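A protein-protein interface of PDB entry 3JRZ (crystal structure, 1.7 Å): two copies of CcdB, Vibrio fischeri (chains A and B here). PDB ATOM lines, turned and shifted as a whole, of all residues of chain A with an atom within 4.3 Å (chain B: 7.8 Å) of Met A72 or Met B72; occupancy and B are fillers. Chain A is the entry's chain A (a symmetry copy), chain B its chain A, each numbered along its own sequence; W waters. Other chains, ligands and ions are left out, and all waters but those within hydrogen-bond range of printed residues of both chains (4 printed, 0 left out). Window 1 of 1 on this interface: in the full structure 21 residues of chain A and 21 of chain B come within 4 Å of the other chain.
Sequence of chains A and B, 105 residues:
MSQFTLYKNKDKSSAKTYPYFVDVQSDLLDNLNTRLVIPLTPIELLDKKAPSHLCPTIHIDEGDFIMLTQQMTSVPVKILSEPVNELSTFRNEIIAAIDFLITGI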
ATOM      1  N   VAL A  24     -12.908   2.237 -11.271  1.00  0.00           N
ATOM      2  CA  VAL A  24     -11.722   1.384 -11.402  1.00  0.00           C
ATOM      3  C   VAL A  24     -10.628   1.980 -12.244  1.00  0.00           C
ATOM      4  O   VAL A  24      -9.651   1.310 -12.563  1.00  0.00           O
ATOM      5  CB  VAL A  24     -12.069  -0.013 -11.923  1.00  0.00           C
ATOM      6  CG1 VAL A  24     -12.986  -0.702 -10.886  1.00  0.00           C
ATOM      7  CG2 VAL A  24     -12.730   0.060 -13.301  1.00  0.00           C
ATOM      8  N   LEU A  36     -13.961   4.868 -15.958  1.00  0.00           N
ATOM      9  CA  LEU A  36     -14.418   3.481 -16.109  1.00  0.00           C
ATOM     10  C   LEU A  36     -14.965   3.041 -14.754  1.00  0.00           C
ATOM     11  O   LEU A  36     -14.249   3.131 -13.778  1.00  0.00           O
ATOM     12  CB  LEU A  36     -13.252   2.592 -16.480  1.00  0.00           C
ATOM     13  CG  LEU A  36     -13.547   1.154 -16.905  1.00  0.00           C
ATOM     14  CD1 LEU A  36     -14.425   1.143 -18.156  1.00  0.00           C
ATOM     15  CD2 LEU A  36     -12.226   0.439 -17.151  1.00  0.00           C
ATOM     16  N   VAL A  37     -16.212   2.552 -14.701  1.00  0.00           N
ATOM     17  CA  VAL A  37     -16.786   2.060 -13.439  1.00  0.00           C
ATOM     18  C   VAL A  37     -17.371   0.658 -13.600  1.00  0.00           C
ATOM     19  O   VAL A  37     -17.693   0.226 -14.714  1.00  0.00           O
ATOM     20  CB  VAL A  37     -17.903   2.988 -12.943  1.00  0.00           C
ATOM     21  CG1 VAL A  37     -17.349   4.415 -12.802  1.00  0.00           C
ATOM     22  CG2 VAL A  37     -19.057   3.006 -13.927  1.00  0.00           C
ATOM     23  N   ILE A  38     -17.534  -0.032 -12.474  1.00  0.00           N
ATOM     24  CA  ILE A  38     -18.184  -1.346 -12.496  1.00  0.00           C
ATOM     25  C   ILE A  38     -19.331  -1.335 -11.507  1.00  0.00           C
ATOM     26  O   ILE A  38     -19.159  -0.918 -10.367  1.00  0.00           O
ATOM     27  CB  ILE A  38     -17.203  -2.471 -12.119  1.00  0.00           C
ATOM     28  CG1 ILE A  38     -16.057  -2.554 -13.124  1.00  0.00           C
ATOM     29  CG2 ILE A  38     -17.920  -3.799 -12.140  1.00  0.00           C
ATOM     30  CD1 ILE A  38     -15.031  -3.593 -12.794  1.00  0.00           C
ATOM     31  N   LEU A  68     -20.343  -6.825 -10.965  1.00  0.00           N
ATOM     32  CA  LEU A  68     -20.646  -7.283 -12.310  1.00  0.00           C
ATOM     33  C   LEU A  68     -19.654  -6.717 -13.317  1.00  0.00           C
ATOM     34  O   LEU A  68     -19.946  -5.790 -14.077  1.00  0.00           O
ATOM     35  CB  LEU A  68     -22.074  -6.915 -12.688  1.00  0.00           C
ATOM     36  CG  LEU A  68     -23.104  -7.586 -11.784  1.00  0.00           C
ATOM     37  CD1 LEU A  68     -24.492  -7.089 -12.155  1.00  0.00           C
ATOM     38  CD2 LEU A  68     -23.015  -9.082 -11.966  1.00  0.00           C
ATOM     39  N   THR A  69     -18.457  -7.279 -13.273  1.00  0.00           N
ATOM     40  CA  THR A  69     -17.342  -6.831 -14.081  1.00  0.00           C
ATOM     41  C   THR A  69     -17.706  -6.747 -15.566  1.00  0.00           C
ATOM     42  O   THR A  69     -17.243  -5.866 -16.268  1.00  0.00           O
ATOM     43  CB  THR A  69     -16.181  -7.810 -13.891  1.00  0.00           C
ATOM     44  OG1 THR A  69     -15.973  -8.027 -12.473  1.00  0.00           O
ATOM     45  CG2 THR A  69     -14.896  -7.276 -14.560  1.00  0.00           C
ATOM     46  N   GLN A  70     -18.526  -7.671 -16.043  1.00  0.00           N
ATOM     47  CA  GLN A  70     -18.873  -7.677 -17.460  1.00  0.00           C
ATOM     48  C   GLN A  70     -19.736  -6.500 -17.883  1.00  0.00           C
ATOM     49  O   GLN A  70     -19.912  -6.268 -19.079  1.00  0.00           O
ATOM     50  CB  GLN A  70     -19.586  -8.980 -17.835  1.00  0.00           C
ATOM     51  CG  GLN A  70     -20.923  -9.168 -17.152  1.00  0.00           C
ATOM     52  CD  GLN A  70     -20.828 -10.031 -15.891  1.00  0.00           C
ATOM     53  OE1 GLN A  70     -21.616 -10.969 -15.699  1.00  0.00           O
ATOM     54  NE2 GLN A  70     -19.871  -9.723 -15.032  1.00  0.00           N
ATOM     55  N   GLN A  71     -20.296  -5.783 -16.908  1.00  0.00           N
ATOM     56  CA  GLN A  71     -21.098  -4.595 -17.182  1.00  0.00           C
ATOM     57  C   GLN A  71     -20.280  -3.322 -16.979  1.00  0.00           C
ATOM     58  O   GLN A  71     -20.862  -2.232 -16.874  1.00  0.00           O
ATOM     59  CB  GLN A  71     -22.325  -4.554 -16.257  1.00  0.00           C
ATOM     60  CG  GLN A  71     -23.292  -5.665 -16.504  1.00  0.00           C
ATOM     61  CD  GLN A  71     -24.324  -5.289 -17.528  1.00  0.00           C
ATOM     62  OE1 GLN A  71     -24.517  -4.102 -17.818  1.00  0.00           O
ATOM     63  NE2 GLN A  71     -25.011  -6.292 -18.078  1.00  0.00           N
ATOM     64  N   MET A  72     -18.950  -3.455 -16.946  1.00  0.00           N
ATOM     65  CA  MET A  72     -18.067  -2.278 -16.817  1.00  0.00           C
ATOM     66  C   MET A  72     -18.393  -1.281 -17.924  1.00  0.00           C
ATOM     67  O   MET A  72     -18.689  -1.664 -19.046  1.00  0.00           O
ATOM     68  CB  MET A  72     -16.600  -2.708 -16.924  1.00  0.00           C
ATOM     69  CG  MET A  72     -15.555  -1.634 -16.567  1.00  0.00           C
ATOM     70  SD  MET A  72     -13.860  -2.315 -16.614  1.00  0.00           S
ATOM     71  CE  MET A  72     -14.108  -3.269 -18.102  1.00  0.00           C
ATOM     72  N   THR A  73     -18.334   0.011 -17.629  1.00  0.00           N
ATOM     73  CA  THR A  73     -18.628   0.982 -18.668  1.00  0.00           C
ATOM     74  C   THR A  73     -18.010   2.324 -18.294  1.00  0.00           C
ATOM     75  O   THR A  73     -17.761   2.574 -17.130  1.00  0.00           O
ATOM     76  CB  THR A  73     -20.144   1.132 -18.876  1.00  0.00           C
ATOM     77  OG1 THR A  73     -20.394   2.054 -19.944  1.00  0.00           O
ATOM     78  CG2 THR A  73     -20.814   1.639 -17.604  1.00  0.00           C
ATOM     79  N   SER A  74     -17.765   3.161 -19.304  1.00  0.00           N
ATOM     80  CA  SER A  74     -17.250   4.520 -19.116  1.00  0.00           C
ATOM     81  C   SER A  74     -18.435   5.449 -18.853  1.00  0.00           C
ATOM     82  O   SER A  74     -19.405   5.455 -19.636  1.00  0.00           O
ATOM     83  CB  SER A  74     -16.587   4.946 -20.438  1.00  0.00           C
ATOM     84  OG  SER A  74     -16.081   6.282 -20.402  1.00  0.00           O
ATOM     85  N   LEU A 101     -11.757 -10.918 -17.627  1.00  0.00           N
ATOM     86  CA  LEU A 101     -12.755 -10.547 -18.631  1.00  0.00           C
ATOM     87  C   LEU A 101     -12.059 -10.352 -19.981  1.00  0.00           C
ATOM     88  O   LEU A 101     -12.627 -10.638 -21.034  1.00  0.00           O
ATOM     89  CB  LEU A 101     -13.469  -9.261 -18.208  1.00  0.00           C
ATOM     90  CG  LEU A 101     -14.424  -8.645 -19.224  1.00  0.00           C
ATOM     91  CD1 LEU A 101     -15.584  -9.585 -19.479  1.00  0.00           C
ATOM     92  CD2 LEU A 101     -14.898  -7.299 -18.647  1.00  0.00           C
ATOM     93  N   VAL B  22     -14.289  -2.283 -31.563  1.00  0.00           N
ATOM     94  CA  VAL B  22     -13.553  -3.560 -31.489  1.00  0.00           C
ATOM     95  C   VAL B  22     -13.989  -4.331 -30.256  1.00  0.00           C
ATOM     96  O   VAL B  22     -14.071  -3.769 -29.152  1.00  0.00           O
ATOM     97  CB  VAL B  22     -12.007  -3.377 -31.527  1.00  0.00           C
ATOM     98  CG1 VAL B  22     -11.527  -2.490 -30.402  1.00  0.00           C
ATOM     99  CG2 VAL B  22     -11.291  -4.728 -31.441  1.00  0.00           C
ATOM    100  N   VAL B  24     -13.238  -6.485 -27.330  1.00  0.00           N
ATOM    101  CA  VAL B  24     -12.015  -6.830 -26.598  1.00  0.00           C
ATOM    102  C   VAL B  24     -12.212  -7.872 -25.532  1.00  0.00           C
ATOM    103  O   VAL B  24     -11.309  -8.137 -24.744  1.00  0.00           O
ATOM    104  CB  VAL B  24     -11.335  -5.598 -25.994  1.00  0.00           C
ATOM    105  CG1 VAL B  24     -10.900  -4.669 -27.151  1.00  0.00           C
ATOM    106  CG2 VAL B  24     -12.265  -4.880 -25.012  1.00  0.00           C
ATOM    107  N   GLN B  25     -13.377  -8.502 -25.521  1.00  0.00           N
ATOM    108  CA  GLN B  25     -13.672  -9.450 -24.452  1.00  0.00           C
ATOM    109  C   GLN B  25     -13.170 -10.855 -24.752  1.00  0.00           C
ATOM    110  O   GLN B  25     -13.224 -11.304 -25.894  1.00  0.00           O
ATOM    111  CB  GLN B  25     -15.171  -9.451 -24.226  1.00  0.00           C
ATOM    112  CG  GLN B  25     -15.666 -10.379 -23.160  1.00  0.00           C
ATOM    113  CD  GLN B  25     -17.080 -10.049 -22.831  1.00  0.00           C
ATOM    114  OE1 GLN B  25     -17.383  -8.924 -22.403  1.00  0.00           O
ATOM    115  NE2 GLN B  25     -17.981 -10.999 -23.084  1.00  0.00           N
ATOM    116  N   THR B  34     -23.469  -9.852 -23.312  1.00  0.00           N
ATOM    117  CA  THR B  34     -22.822  -8.561 -23.564  1.00  0.00           C
ATOM    118  C   THR B  34     -21.371  -8.754 -24.013  1.00  0.00           C
ATOM    119  O   THR B  34     -20.766  -9.805 -23.755  1.00  0.00           O
ATOM    120  CB  THR B  34     -22.797  -7.717 -22.284  1.00  0.00           C
ATOM    121  OG1 THR B  34     -22.257  -8.502 -21.225  1.00  0.00           O
ATOM    122  CG2 THR B  34     -24.209  -7.308 -21.903  1.00  0.00           C
ATOM    123  N   ARG B  35     -20.811  -7.737 -24.675  1.00  0.00           N
ATOM    124  CA  ARG B  35     -19.376  -7.746 -24.995  1.00  0.00           C
ATOM    125  C   ARG B  35     -18.763  -6.412 -24.605  1.00  0.00           C
ATOM    126  O   ARG B  35     -19.356  -5.373 -24.875  1.00  0.00           O
ATOM    127  CB  ARG B  35     -19.160  -7.925 -26.496  1.00  0.00           C
ATOM    128  CG  ARG B  35     -19.720  -9.239 -27.032  1.00  0.00           C
ATOM    129  CD  ARG B  35     -18.815 -10.400 -26.664  1.00  0.00           C
ATOM    130  NE  ARG B  35     -19.295 -11.632 -27.299  1.00  0.00           N
ATOM    131  CZ  ARG B  35     -20.197 -12.429 -26.737  1.00  0.00           C
ATOM    132  NH1 ARG B  35     -20.578 -13.518 -27.376  1.00  0.00           N
ATOM    133  NH2 ARG B  35     -20.688 -12.155 -25.528  1.00  0.00           N
ATOM    134  N   LEU B  36     -17.577  -6.434 -23.988  1.00  0.00           N
ATOM    135  CA  LEU B  36     -16.823  -5.195 -23.764  1.00  0.00           C
ATOM    136  C   LEU B  36     -16.260  -4.762 -25.114  1.00  0.00           C
ATOM    137  O   LEU B  36     -15.580  -5.547 -25.742  1.00  0.00           O
ATOM    138  CB  LEU B  36     -15.675  -5.457 -22.815  1.00  0.00           C
ATOM    139  CG  LEU B  36     -14.900  -4.258 -22.270  1.00  0.00           C
ATOM    140  CD1 LEU B  36     -15.830  -3.347 -21.471  1.00  0.00           C
ATOM    141  CD2 LEU B  36     -13.753  -4.770 -21.409  1.00  0.00           C
ATOM    142  N   VAL B  37     -16.526  -3.521 -25.545  1.00  0.00           N
ATOM    143  CA  VAL B  37     -15.974  -3.018 -26.813  1.00  0.00           C
ATOM    144  C   VAL B  37     -15.279  -1.671 -26.625  1.00  0.00           C
ATOM    145  O   VAL B  37     -15.545  -0.946 -25.657  1.00  0.00           O
ATOM    146  CB  VAL B  37     -17.079  -2.841 -27.863  1.00  0.00           C
ATOM    147  CG1 VAL B  37     -17.817  -4.177 -28.050  1.00  0.00           C
ATOM    148  CG2 VAL B  37     -18.075  -1.790 -27.416  1.00  0.00           C
ATOM    149  N   ILE B  38     -14.411  -1.331 -27.575  1.00  0.00           N
ATOM    150  CA  ILE B  38     -13.764  -0.016 -27.553  1.00  0.00           C
ATOM    151  C   ILE B  38     -14.000   0.661 -28.888  1.00  0.00           C
ATOM    152  O   ILE B  38     -13.791   0.055 -29.933  1.00  0.00           O
ATOM    153  CB  ILE B  38     -12.250  -0.132 -27.308  1.00  0.00           C
ATOM    154  CG1 ILE B  38     -11.965  -0.761 -25.945  1.00  0.00           C
ATOM    155  CG2 ILE B  38     -11.626   1.242 -27.310  1.00  0.00           C
ATOM    156  CD1 ILE B  38     -10.509  -0.956 -25.656  1.00  0.00           C
ATOM    157  N   PRO B  39     -14.448   1.930 -28.878  1.00  0.00           N
ATOM    158  CA  PRO B  39     -14.692   2.592 -30.166  1.00  0.00           C
ATOM    159  C   PRO B  39     -13.413   3.101 -30.843  1.00  0.00           C
ATOM    160  O   PRO B  39     -12.424   3.439 -30.177  1.00  0.00           O
ATOM    161  CB  PRO B  39     -15.566   3.800 -29.791  1.00  0.00           C
ATOM    162  CG  PRO B  39     -15.231   4.098 -28.347  1.00  0.00           C
ATOM    163  CD  PRO B  39     -14.816   2.762 -27.709  1.00  0.00           C
ATOM    164  N   LEU B  68     -10.157   4.743 -28.723  1.00  0.00           N
ATOM    165  CA  LEU B  68     -10.482   5.513 -27.535  1.00  0.00           C
ATOM    166  C   LEU B  68     -10.773   4.598 -26.352  1.00  0.00           C
ATOM    167  O   LEU B  68     -11.920   4.388 -25.952  1.00  0.00           O
ATOM    168  CB  LEU B  68     -11.659   6.441 -27.806  1.00  0.00           C
ATOM    169  CG  LEU B  68     -11.347   7.469 -28.890  1.00  0.00           C
ATOM    170  CD1 LEU B  68     -12.598   8.284 -29.178  1.00  0.00           C
ATOM    171  CD2 LEU B  68     -10.234   8.367 -28.408  1.00  0.00           C
ATOM    172  N   THR B  69      -9.699   4.031 -25.829  1.00  0.00           N
ATOM    173  CA  THR B  69      -9.759   3.058 -24.758  1.00  0.00           C
ATOM    174  C   THR B  69     -10.580   3.563 -23.570  1.00  0.00           C
ATOM    175  O   THR B  69     -11.273   2.797 -22.924  1.00  0.00           O
ATOM    176  CB  THR B  69      -8.331   2.750 -24.303  1.00  0.00           C
ATOM    177  OG1 THR B  69      -7.516   2.458 -25.465  1.00  0.00           O
ATOM    178  CG2 THR B  69      -8.314   1.568 -23.309  1.00  0.00           C
ATOM    179  N   GLN B  70     -10.492   4.852 -23.275  1.00  0.00           N
ATOM    180  CA  GLN B  70     -11.211   5.388 -22.124  1.00  0.00           C
ATOM    181  C   GLN B  70     -12.721   5.391 -22.294  1.00  0.00           C
ATOM    182  O   GLN B  70     -13.446   5.607 -21.322  1.00  0.00           O
ATOM    183  CB  GLN B  70     -10.740   6.812 -21.810  1.00  0.00           C
ATOM    184  CG  GLN B  70     -11.042   7.814 -22.901  1.00  0.00           C
ATOM    185  CD  GLN B  70      -9.856   8.040 -23.843  1.00  0.00           C
ATOM    186  OE1 GLN B  70      -9.485   9.186 -24.139  1.00  0.00           O
ATOM    187  NE2 GLN B  70      -9.257   6.959 -24.313  1.00  0.00           N
ATOM    188  N   GLN B  71     -13.189   5.185 -23.525  1.00  0.00           N
ATOM    189  CA  GLN B  71     -14.619   5.107 -23.808  1.00  0.00           C
ATOM    190  C   GLN B  71     -15.077   3.655 -23.921  1.00  0.00           C
ATOM    191  O   GLN B  71     -16.172   3.400 -24.445  1.00  0.00           O
ATOM    192  CB  GLN B  71     -14.944   5.838 -25.120  1.00  0.00           C
ATOM    193  CG  GLN B  71     -14.705   7.311 -25.055  1.00  0.00           C
ATOM    194  CD  GLN B  71     -15.924   8.055 -24.593  1.00  0.00           C
ATOM    195  OE1 GLN B  71     -17.038   7.518 -24.629  1.00  0.00           O
ATOM    196  NE2 GLN B  71     -15.734   9.305 -24.166  1.00  0.00           N
ATOM    197  N   MET B  72     -14.263   2.721 -23.419  1.00  0.00           N
ATOM    198  CA  MET B  72     -14.642   1.294 -23.422  1.00  0.00           C
ATOM    199  C   MET B  72     -15.993   1.131 -22.734  1.00  0.00           C
ATOM    200  O   MET B  72     -16.285   1.807 -21.759  1.00  0.00           O
ATOM    201  CB  MET B  72     -13.582   0.468 -22.685  1.00  0.00           C
ATOM    202  CG  MET B  72     -13.711  -1.062 -22.813  1.00  0.00           C
ATOM    203  SD  MET B  72     -12.318  -1.916 -21.995  1.00  0.00           S
ATOM    204  CE  MET B  72     -12.292  -0.852 -20.563  1.00  0.00           C
ATOM    205  N   THR B  73     -16.830   0.227 -23.223  1.00  0.00           N
ATOM    206  CA  THR B  73     -18.120   0.043 -22.579  1.00  0.00           C
ATOM    207  C   THR B  73     -18.670  -1.333 -22.936  1.00  0.00           C
ATOM    208  O   THR B  73     -18.285  -1.898 -23.942  1.00  0.00           O
ATOM    209  CB  THR B  73     -19.112   1.140 -22.997  1.00  0.00           C
ATOM    210  OG1 THR B  73     -20.350   0.959 -22.301  1.00  0.00           O
ATOM    211  CG2 THR B  73     -19.365   1.092 -24.500  1.00  0.00           C
ATOM    212  N   SER B  74     -19.561  -1.848 -22.088  1.00  0.00           N
ATOM    213  CA  SER B  74     -20.251  -3.120 -22.319  1.00  0.00           C
ATOM    214  C   SER B  74     -21.481  -2.848 -23.185  1.00  0.00           C
ATOM    215  O   SER B  74     -22.295  -1.967 -22.847  1.00  0.00           O
ATOM    216  CB  SER B  74     -20.729  -3.638 -20.951  1.00  0.00           C
ATOM    217  OG  SER B  74     -21.462  -4.861 -21.044  1.00  0.00           O
ATOM    218  N   VAL B  75     -21.661  -3.632 -24.251  1.00  0.00           N
ATOM    219  CA  VAL B  75     -22.854  -3.504 -25.101  1.00  0.00           C
ATOM    220  C   VAL B  75     -23.510  -4.862 -25.306  1.00  0.00           C
ATOM    221  O   VAL B  75     -22.871  -5.886 -25.093  1.00  0.00           O
ATOM    222  CB  VAL B  75     -22.529  -2.935 -26.472  1.00  0.00           C
ATOM    223  CG1 VAL B  75     -21.843  -1.583 -26.336  1.00  0.00           C
ATOM    224  CG2 VAL B  75     -21.630  -3.891 -27.253  1.00  0.00           C
ATOM    225  N   ILE B  94      -3.248  -3.160 -27.820  1.00  0.00           N
ATOM    226  CA  ILE B  94      -4.627  -2.977 -27.320  1.00  0.00           C
ATOM    227  C   ILE B  94      -4.700  -3.370 -25.848  1.00  0.00           C
ATOM    228  O   ILE B  94      -5.187  -2.625 -25.007  1.00  0.00           O
ATOM    229  CB  ILE B  94      -5.614  -3.824 -28.161  1.00  0.00           C
ATOM    230  CG1 ILE B  94      -5.698  -3.249 -29.578  1.00  0.00           C
ATOM    231  CG2 ILE B  94      -6.993  -3.894 -27.489  1.00  0.00           C
ATOM    232  CD1 ILE B  94      -6.556  -4.094 -30.545  1.00  0.00           C
ATOM    233  N   ALA B  97      -2.937  -0.883 -23.629  1.00  0.00           N
ATOM    234  CA  ALA B  97      -3.696   0.348 -23.441  1.00  0.00           C
ATOM    235  C   ALA B  97      -4.732   0.149 -22.356  1.00  0.00           C
ATOM    236  O   ALA B  97      -4.966   1.016 -21.547  1.00  0.00           O
ATOM    237  CB  ALA B  97      -4.377   0.764 -24.716  1.00  0.00           C
ATOM    238  N   ILE B  98      -5.415  -0.985 -22.385  1.00  0.00           N
ATOM    239  CA  ILE B  98      -6.401  -1.256 -21.337  1.00  0.00           C
ATOM    240  C   ILE B  98      -5.695  -1.368 -19.991  1.00  0.00           C
ATOM    241  O   ILE B  98      -6.181  -0.849 -18.988  1.00  0.00           O
ATOM    242  CB  ILE B  98      -7.184  -2.554 -21.622  1.00  0.00           C
ATOM    243  CG1 ILE B  98      -7.973  -2.427 -22.933  1.00  0.00           C
ATOM    244  CG2 ILE B  98      -8.116  -2.899 -20.451  1.00  0.00           C
ATOM    245  CD1 ILE B  98      -8.550  -3.779 -23.442  1.00  0.00           C
ATOM    246  N   LEU B 101      -5.062   2.032 -18.646  1.00  0.00           N
ATOM    247  CA  LEU B 101      -6.253   2.749 -18.188  1.00  0.00           C
ATOM    248  C   LEU B 101      -6.548   2.355 -16.739  1.00  0.00           C
ATOM    249  O   LEU B 101      -7.032   3.164 -15.948  1.00  0.00           O
ATOM    250  CB  LEU B 101      -7.445   2.411 -19.087  1.00  0.00           C
ATOM    251  CG  LEU B 101      -8.803   2.946 -18.649  1.00  0.00           C
ATOM    252  CD1 LEU B 101      -8.797   4.460 -18.682  1.00  0.00           C
ATOM    253  CD2 LEU B 101      -9.855   2.359 -19.606  1.00  0.00           C
ATOM    254  N   ILE B 102      -6.248   1.103 -16.404  1.00  0.00           N
ATOM    255  CA  ILE B 102      -6.584   0.557 -15.091  1.00  0.00           C
ATOM    256  C   ILE B 102      -5.440   0.628 -14.109  1.00  0.00           C
ATOM    257  O   ILE B 102      -5.639   0.977 -12.952  1.00  0.00           O
ATOM    258  CB  ILE B 102      -7.117  -0.869 -15.231  1.00  0.00           C
ATOM    259  CG1 ILE B 102      -8.400  -0.826 -16.056  1.00  0.00           C
ATOM    260  CG2 ILE B 102      -7.391  -1.477 -13.866  1.00  0.00           C
ATOM    261  CD1 ILE B 102      -8.765  -2.139 -16.667  1.00  0.00           C
HETATM  262  O   HOH W   1     -20.171   4.249 -22.188  1.00  0.00           O
HETATM  263  O   HOH W   2     -22.756  -0.151 -20.601  1.00  0.00           O
HETATM  264  O   HOH W   3     -19.675  -7.842 -21.269  1.00  0.00           O
HETATM  265  O   HOH W   4     -12.960   6.822 -18.952  1.00  0.00           O
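The side-chain hydroxyl of Ser A74 is in hydrogen-bond range of the backbone carbonyl oxygen of Gln B70.
The backbone carbonyl oxygen of Met B72 is in hydrogen-bond range of the backbone NH of Ser A74, at 3.2 Å.
OG1 of Thr B73 sits at hydrogen-bond distance from OG1 of Thr A73, at 2.6 Å.
OG of Ser B74 lies within hydrogen-bond range of O of Gln A70 (2.9 Å).
The backbone NH of Ser B74 sits at hydrogen-bond distance from the backbone carbonyl oxygen of Met A72, 3.2 Å away.
N of Val B24 is in hydrogen-bond range of O of Leu B36.
The backbone carbonyl oxygen (O) of Thr B34 lies within hydrogen-bond range of the side-chain amide nitrogen (NE2) of Gln B25 (3.1 Å).
The side-chain amide oxygen (OE1) of Gln B25 sits at hydrogen-bond distance from the backbone NH (N) of Leu B36.
The backbone NH (N) of Val B37 sits at hydrogen-bond distance from the backbone carbonyl oxygen (O) of Thr B73, 2.9 Å away.
The backbone NH (N) of Val A24 lies within hydrogen-bond range of the backbone carbonyl oxygen (O) of Leu A36 (3.0 Å).
O of Thr A73 lies within hydrogen-bond range of N of Val A37.
Among the printed residues, merely in contact across the chains: Leu A101 with Gln B25, Leu A36 with Met B72, Met A72 with Leu B36, Val A24 with Ile B102, Gln A70 with Thr B34, Gln A71 with Ser B74, Ser A74 with Gln B71, Met A72 with Met B72, Met A72 with Thr B73, Thr A73 with Met B72, Leu A36 with Leu B101 and Leu A101 with Leu B36.
Met A72 touches four residues of chain B.
Printed residues of chain A within 4 Å of Met B72: Leu A36 (3.6 Å), Met A72 (3.9 Å), Thr A73 (3.9 Å) and Ser A74 (3.2 Å).
Of the printed residues of chain B, Leu A36 touches Met B72 and Leu B101.
Printed residues of chain A within 4 Å of Thr B73: Met A72 (3.9 Å) and Thr A73 (2.6 Å).
Printed residues of chain B within 4 Å of Leu A101: Gln B25 (3.5 Å) and Leu B36 (3.9 Å).
Val B22 touches none of the printed residues of chain A.
The nearest printed residue of chain A that does not touch Ser B74 is Thr A73 (4.4 Å).
Hydrophobic or aromatic side chains of chain B that line the printed part of chain A: Leu B36, Met B72, Leu B101 and Ile B102.
Of the 12 printed residues of chain A, 8 touch a printed residue of chain B.
Hydrophobic or aromatic side chains of chain A that line the printed part of chain B: Leu A36, Met A72 and Leu A101.
Among the printed residues, 17 pairs touch across the chains.
Leu A36 touches Met B72, and with the chains exchanged Met A72 touches Leu B36.
Leu A36 touches Leu B101, and with the chains exchanged Leu A101 touches Leu B36.
Met A72 touches Thr B73, and with the chains exchanged Thr A73 touches Met B72.
Met A72 touches Ser B74, and with the chains exchanged Ser A74 touches Met B72.
Of the 17 pairs that touch across the chains among the printed residues, 14 have their exchanged pair printed and touching as well.
Water W3 lies within hydrogen-bond range of the side-chain hydroxyl of Thr B34 (2.7 Å), the backbone carbonyl oxygen of Gln A70 (2.7 Å), the side-chain amide oxygen of Gln B25 (2.8 Å) and the side-chain hydroxyl of Ser B74 (3.5 Å).
Water W4 lies within hydrogen-bond range of the backbone carbonyl oxygen (O) of Gln B70 (2.7 Å) and the side-chain hydroxyl (OG) of Ser A74 (3.5 Å).
Water W2 lies within hydrogen-bond range of the backbone carbonyl oxygen (O) of Ser B74 (2.9 Å), the side-chain hydroxyl (OG1) of Thr B73 (3.1 Å) and the side-chain hydroxyl (OG1) of Thr A73 (3.3 Å).
Water W1 lies within hydrogen-bond range of O of Ser A74, OG1 of Thr A73 and OG1 of Thr B73.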
